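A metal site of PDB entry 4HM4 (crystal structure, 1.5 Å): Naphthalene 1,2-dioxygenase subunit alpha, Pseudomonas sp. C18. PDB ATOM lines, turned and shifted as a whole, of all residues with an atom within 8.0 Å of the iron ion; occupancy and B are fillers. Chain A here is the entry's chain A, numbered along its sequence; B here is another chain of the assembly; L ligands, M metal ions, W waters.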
ATOM      1  N   ASN A 201       8.927  16.970 -26.759  1.00  0.00           N
ATOM      2  CA  ASN A 201       7.968  17.628 -25.873  1.00  0.00           C
ATOM      3  C   ASN A 201       8.625  18.812 -25.177  1.00  0.00           C
ATOM      4  O   ASN A 201       8.080  19.923 -25.172  1.00  0.00           O
ATOM      5  CB  ASN A 201       7.414  16.600 -24.880  1.00  0.00           C
ATOM      6  CG  ASN A 201       6.401  17.201 -23.919  1.00  0.00           C
ATOM      7  OD1 ASN A 201       5.192  17.201 -24.194  1.00  0.00           O
ATOM      8  ND2 ASN A 201       6.876  17.716 -22.803  1.00  0.00           N
ATOM      9  N   PHE A 202       9.809  18.607 -24.614  1.00  0.00           N
ATOM     10  CA  PHE A 202      10.525  19.682 -23.946  1.00  0.00           C
ATOM     11  C   PHE A 202      11.070  20.748 -24.887  1.00  0.00           C
ATOM     12  O   PHE A 202      11.179  21.906 -24.491  1.00  0.00           O
ATOM     13  CB  PHE A 202      11.657  19.129 -23.069  1.00  0.00           C
ATOM     14  CG  PHE A 202      11.187  18.671 -21.709  1.00  0.00           C
ATOM     15  CD1 PHE A 202      10.298  17.607 -21.588  1.00  0.00           C
ATOM     16  CD2 PHE A 202      11.653  19.293 -20.558  1.00  0.00           C
ATOM     17  CE1 PHE A 202       9.862  17.177 -20.331  1.00  0.00           C
ATOM     18  CE2 PHE A 202      11.226  18.859 -19.287  1.00  0.00           C
ATOM     19  CZ  PHE A 202      10.323  17.807 -19.182  1.00  0.00           C
ATOM     20  N   ASP A 205       6.959  22.081 -27.063  1.00  0.00           N
ATOM     21  CA  ASP A 205       5.545  21.782 -26.875  1.00  0.00           C
ATOM     22  C   ASP A 205       4.902  22.555 -25.733  1.00  0.00           C
ATOM     23  O   ASP A 205       4.772  22.039 -24.628  1.00  0.00           O
ATOM     24  CB  ASP A 205       5.354  20.283 -26.660  1.00  0.00           C
ATOM     25  CG  ASP A 205       3.910  19.833 -26.786  1.00  0.00           C
ATOM     26  OD1 ASP A 205       2.986  20.673 -26.737  1.00  0.00           O
ATOM     27  OD2 ASP A 205       3.712  18.608 -26.899  1.00  0.00           O
ATOM     28  N   HIS A 208       0.599  21.436 -25.379  1.00  0.00           N
ATOM     29  CA  HIS A 208       0.063  20.358 -24.542  1.00  0.00           C
ATOM     30  C   HIS A 208      -0.230  20.755 -23.096  1.00  0.00           C
ATOM     31  O   HIS A 208      -1.010  20.094 -22.417  1.00  0.00           O
ATOM     32  CB  HIS A 208       1.002  19.132 -24.553  1.00  0.00           C
ATOM     33  CG  HIS A 208       2.079  19.173 -23.516  1.00  0.00           C
ATOM     34  ND1 HIS A 208       3.162  20.033 -23.590  1.00  0.00           N
ATOM     35  CD2 HIS A 208       2.252  18.455 -22.390  1.00  0.00           C
ATOM     36  CE1 HIS A 208       3.940  19.835 -22.542  1.00  0.00           C
ATOM     37  NE2 HIS A 208       3.414  18.891 -21.800  1.00  0.00           N
ATOM     38  N   VAL A 209       0.392  21.835 -22.620  1.00  0.00           N
ATOM     39  CA  VAL A 209       0.414  22.127 -21.185  1.00  0.00           C
ATOM     40  C   VAL A 209      -0.965  22.266 -20.537  1.00  0.00           C
ATOM     41  O   VAL A 209      -1.252  21.590 -19.538  1.00  0.00           O
ATOM     42  CB  VAL A 209       1.299  23.345 -20.843  1.00  0.00           C
ATOM     43  CG1 VAL A 209       1.244  23.636 -19.340  1.00  0.00           C
ATOM     44  CG2 VAL A 209       2.736  23.097 -21.286  1.00  0.00           C
ATOM     45  N   THR A 212      -2.871  18.432 -21.226  1.00  0.00           N
ATOM     46  CA  THR A 212      -2.150  17.335 -20.564  1.00  0.00           C
ATOM     47  C   THR A 212      -2.037  17.563 -19.059  1.00  0.00           C
ATOM     48  O   THR A 212      -2.311  16.662 -18.258  1.00  0.00           O
ATOM     49  CB  THR A 212      -0.722  17.177 -21.144  1.00  0.00           C
ATOM     50  OG1 THR A 212      -0.794  16.604 -22.451  1.00  0.00           O
ATOM     51  CG2 THR A 212       0.111  16.264 -20.274  1.00  0.00           C
ATOM     52  N   HIS A 213      -1.659  18.776 -18.672  1.00  0.00           N
ATOM     53  CA  HIS A 213      -1.355  19.066 -17.277  1.00  0.00           C
ATOM     54  C   HIS A 213      -2.485  19.794 -16.563  1.00  0.00           C
ATOM     55  O   HIS A 213      -2.256  20.428 -15.537  1.00  0.00           O
ATOM     56  CB  HIS A 213      -0.053  19.866 -17.160  1.00  0.00           C
ATOM     57  CG  HIS A 213       1.157  19.121 -17.625  1.00  0.00           C
ATOM     58  ND1 HIS A 213       1.668  18.028 -16.952  1.00  0.00           N
ATOM     59  CD2 HIS A 213       1.972  19.314 -18.698  1.00  0.00           C
ATOM     60  CE1 HIS A 213       2.737  17.572 -17.588  1.00  0.00           C
ATOM     61  NE2 HIS A 213       2.938  18.338 -18.654  1.00  0.00           N
ATOM     62  N   LEU A 307      13.893  22.773 -17.892  1.00  0.00           N
ATOM     63  CA  LEU A 307      12.996  23.888 -17.702  1.00  0.00           C
ATOM     64  C   LEU A 307      13.730  24.857 -16.800  1.00  0.00           C
ATOM     65  O   LEU A 307      13.886  24.577 -15.603  1.00  0.00           O
ATOM     66  CB  LEU A 307      11.712  23.443 -17.009  1.00  0.00           C
ATOM     67  CG  LEU A 307      10.912  22.300 -17.635  1.00  0.00           C
ATOM     68  CD1 LEU A 307       9.671  21.952 -16.794  1.00  0.00           C
ATOM     69  CD2 LEU A 307      10.502  22.624 -19.067  1.00  0.00           C
ATOM     70  N   PHE A 352       8.449  16.950 -11.163  1.00  0.00           N
ATOM     71  CA  PHE A 352       8.970  16.273 -12.353  1.00  0.00           C
ATOM     72  C   PHE A 352       9.895  15.082 -12.091  1.00  0.00           C
ATOM     73  O   PHE A 352      10.465  14.522 -13.024  1.00  0.00           O
ATOM     74  CB  PHE A 352       9.675  17.284 -13.283  1.00  0.00           C
ATOM     75  CG  PHE A 352       8.726  18.042 -14.170  1.00  0.00           C
ATOM     76  CD1 PHE A 352       8.116  19.207 -13.728  1.00  0.00           C
ATOM     77  CD2 PHE A 352       8.408  17.563 -15.431  1.00  0.00           C
ATOM     78  CE1 PHE A 352       7.230  19.897 -14.533  1.00  0.00           C
ATOM     79  CE2 PHE A 352       7.526  18.254 -16.245  1.00  0.00           C
ATOM     80  CZ  PHE A 352       6.929  19.416 -15.799  1.00  0.00           C
ATOM     81  N   TRP A 358       3.393  16.288 -12.174  1.00  0.00           N
ATOM     82  CA  TRP A 358       3.339  16.842 -13.521  1.00  0.00           C
ATOM     83  C   TRP A 358       3.870  15.821 -14.535  1.00  0.00           C
ATOM     84  O   TRP A 358       3.211  15.531 -15.534  1.00  0.00           O
ATOM     85  CB  TRP A 358       4.166  18.116 -13.652  1.00  0.00           C
ATOM     86  CG  TRP A 358       3.637  19.335 -12.957  1.00  0.00           C
ATOM     87  CD1 TRP A 358       3.508  19.521 -11.602  1.00  0.00           C
ATOM     88  CD2 TRP A 358       3.220  20.554 -13.569  1.00  0.00           C
ATOM     89  NE1 TRP A 358       3.016  20.787 -11.347  1.00  0.00           N
ATOM     90  CE2 TRP A 358       2.841  21.434 -12.542  1.00  0.00           C
ATOM     91  CE3 TRP A 358       3.140  20.989 -14.901  1.00  0.00           C
ATOM     92  CZ2 TRP A 358       2.364  22.723 -12.790  1.00  0.00           C
ATOM     93  CZ3 TRP A 358       2.668  22.269 -15.147  1.00  0.00           C
ATOM     94  CH2 TRP A 358       2.289  23.117 -14.100  1.00  0.00           C
ATOM     95  N   GLU A 359       5.054  15.283 -14.276  1.00  0.00           N
ATOM     96  CA  GLU A 359       5.668  14.328 -15.193  1.00  0.00           C
ATOM     97  C   GLU A 359       4.758  13.123 -15.427  1.00  0.00           C
ATOM     98  O   GLU A 359       4.710  12.563 -16.523  1.00  0.00           O
ATOM     99  CB  GLU A 359       7.049  13.883 -14.658  1.00  0.00           C
ATOM    100  CG  GLU A 359       7.756  12.820 -15.495  1.00  0.00           C
ATOM    101  CD  GLU A 359       8.920  13.376 -16.300  1.00  0.00           C
ATOM    102  OE1 GLU A 359       8.911  14.581 -16.632  1.00  0.00           O
ATOM    103  OE2 GLU A 359       9.845  12.589 -16.611  1.00  0.00           O
ATOM    104  N   SER A 360       4.023  12.736 -14.389  1.00  0.00           N
ATOM    105  CA  SER A 360       3.122  11.598 -14.531  1.00  0.00           C
ATOM    106  C   SER A 360       2.032  11.865 -15.578  1.00  0.00           C
ATOM    107  O   SER A 360       1.588  10.933 -16.249  1.00  0.00           O
ATOM    108  CB  SER A 360       2.513  11.197 -13.174  1.00  0.00           C
ATOM    109  OG  SER A 360       1.431  12.029 -12.799  1.00  0.00           O
ATOM    110  N   ASP A 361       1.642  13.139 -15.733  1.00  0.00           N
ATOM    111  CA  ASP A 361       0.619  13.503 -16.729  1.00  0.00           C
ATOM    112  C   ASP A 361       1.069  13.159 -18.150  1.00  0.00           C
ATOM    113  O   ASP A 361       0.234  12.948 -19.026  1.00  0.00           O
ATOM    114  CB  ASP A 361       0.306  15.008 -16.696  1.00  0.00           C
ATOM    115  CG  ASP A 361      -0.243  15.491 -15.357  1.00  0.00           C
ATOM    116  OD1 ASP A 361      -0.860  14.716 -14.606  1.00  0.00           O
ATOM    117  OD2 ASP A 361      -0.076  16.701 -15.075  1.00  0.00           O
ATOM    118  N   ASP A 362       2.377  13.141 -18.361  1.00  0.00           N
ATOM    119  CA  ASP A 362       2.941  12.938 -19.701  1.00  0.00           C
ATOM    120  C   ASP A 362       3.150  11.472 -20.056  1.00  0.00           C
ATOM    121  O   ASP A 362       3.353  11.161 -21.221  1.00  0.00           O
ATOM    122  CB  ASP A 362       4.301  13.639 -19.825  1.00  0.00           C
ATOM    123  CG  ASP A 362       4.190  15.139 -19.848  1.00  0.00           C
ATOM    124  OD1 ASP A 362       3.609  15.671 -20.809  1.00  0.00           O
ATOM    125  OD2 ASP A 362       4.709  15.793 -18.921  1.00  0.00           O
ATOM    126  N   ASN A 363       3.112  10.581 -19.065  1.00  0.00           N
ATOM    127  CA  ASN A 363       3.471   9.169 -19.279  1.00  0.00           C
ATOM    128  C   ASN A 363       2.750   8.520 -20.446  1.00  0.00           C
ATOM    129  O   ASN A 363       3.384   8.045 -21.395  1.00  0.00           O
ATOM    130  CB  ASN A 363       3.200   8.307 -18.030  1.00  0.00           C
ATOM    131  CG  ASN A 363       4.243   8.502 -16.943  1.00  0.00           C
ATOM    132  OD1 ASN A 363       4.053   8.024 -15.815  1.00  0.00           O
ATOM    133  ND2 ASN A 363       5.339   9.178 -17.255  1.00  0.00           N
ATOM    134  N   ASN A 365       0.903   9.770 -22.810  1.00  0.00           N
ATOM    135  CA  ASN A 365       1.190  10.490 -24.051  1.00  0.00           C
ATOM    136  C   ASN A 365       2.483  10.013 -24.705  1.00  0.00           C
ATOM    137  O   ASN A 365       2.495   9.632 -25.877  1.00  0.00           O
ATOM    138  CB  ASN A 365       1.265  12.005 -23.796  1.00  0.00           C
ATOM    139  CG  ASN A 365      -0.068  12.612 -23.362  1.00  0.00           C
ATOM    140  OD1 ASN A 365      -1.136  12.069 -23.648  1.00  0.00           O
ATOM    141  ND2 ASN A 365      -0.008  13.750 -22.676  1.00  0.00           N
ATOM    142  N   MET A 366       3.574  10.020 -23.941  1.00  0.00           N
ATOM    143  CA  MET A 366       4.877   9.619 -24.460  1.00  0.00           C
ATOM    144  C   MET A 366       4.929   8.150 -24.827  1.00  0.00           C
ATOM    145  O   MET A 366       5.453   7.768 -25.883  1.00  0.00           O
ATOM    146  CB  MET A 366       5.974   9.828 -23.407  1.00  0.00           C
ATOM    147  CG  MET A 366       5.965  11.153 -22.704  1.00  0.00           C
ATOM    148  SD  MET A 366       6.756  12.369 -23.720  1.00  0.00           S
ATOM    149  CE  MET A 366       5.309  13.133 -24.442  1.00  0.00           C
ATOM    150  N   TYR B 103      -3.491  14.498 -25.204  1.00  0.00           N
ATOM    151  CA  TYR B 103      -2.192  15.135 -25.352  1.00  0.00           C
ATOM    152  C   TYR B 103      -2.392  16.638 -25.609  1.00  0.00           C
ATOM    153  O   TYR B 103      -2.132  17.448 -24.711  1.00  0.00           O
ATOM    154  CB  TYR B 103      -1.369  14.444 -26.448  1.00  0.00           C
ATOM    155  CG  TYR B 103       0.137  14.681 -26.406  1.00  0.00           C
ATOM    156  CD1 TYR B 103       0.687  15.696 -25.630  1.00  0.00           C
ATOM    157  CD2 TYR B 103       1.004  13.885 -27.141  1.00  0.00           C
ATOM    158  CE1 TYR B 103       2.057  15.919 -25.604  1.00  0.00           C
ATOM    159  CE2 TYR B 103       2.377  14.086 -27.117  1.00  0.00           C
ATOM    160  CZ  TYR B 103       2.899  15.116 -26.360  1.00  0.00           C
ATOM    161  OH  TYR B 103       4.262  15.321 -26.349  1.00  0.00           O
HETATM  162  C1  LIG L   1       6.049  23.086 -18.747  1.00  0.00           C
HETATM  163  C2  LIG L   1       5.864  24.431 -18.868  1.00  0.00           C
HETATM  164  C3  LIG L   1       6.491  22.399 -19.848  1.00  0.00           C
HETATM  165  C4  LIG L   1       6.717  20.930 -19.846  1.00  0.00           C
HETATM  166  C5  LIG L   1       7.447  20.735 -21.171  1.00  0.00           C
HETATM  167  C6  LIG L   1       7.190  21.936 -22.067  1.00  0.00           C
HETATM  168  C7  LIG L   1       6.717  22.958 -21.044  1.00  0.00           C
HETATM  169  C8  LIG L   1       6.534  24.300 -21.197  1.00  0.00           C
HETATM  170  C9  LIG L   1       6.129  25.022 -20.091  1.00  0.00           C
HETATM  171 FE    FE M   1       4.194  17.798 -20.152  1.00  0.00          FE
HETATM  172  O   HOH W   1       6.115  17.978 -20.499  1.00  0.00           O
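ND1 of His 213 lies close to O of Trp 358.
OD2 of Asp 361 lies within hydrogen-bond range of ND1 of His 213, at 2.9 Å.
NE2 of His 208 lies close to OD1 of Asn 201 (3.4 Å).
The backbone carbonyl oxygen of His 208 lies close to the side-chain hydroxyl of Thr 212 (3.5 Å).
A ring nitrogen (ND1) of His 208 lies within hydrogen-bond range of the backbone carbonyl oxygen (O) of Asp 205 (2.8 Å).
OD1 of Asn 201 lies within hydrogen-bond range of OH of Tyr 103 of chain B (3.0 Å).
OD1 of Asn 201 lies close to OD2 of Asp 205 (3.4 Å).
Residues that only touch the iron ion: Asn 201 (3.8 Å).
Within 4 Å of the iron ion: Asn 201, His 208, His 213 and Asp 362.
The iron ion is bound by water W1, a ring nitrogen (NE2) of His 213, a ring nitrogen (NE2) of His 208, the side-chain carboxylate (OD1) of Asp 362 and the side-chain carboxylate (OD2) of Asp 362.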
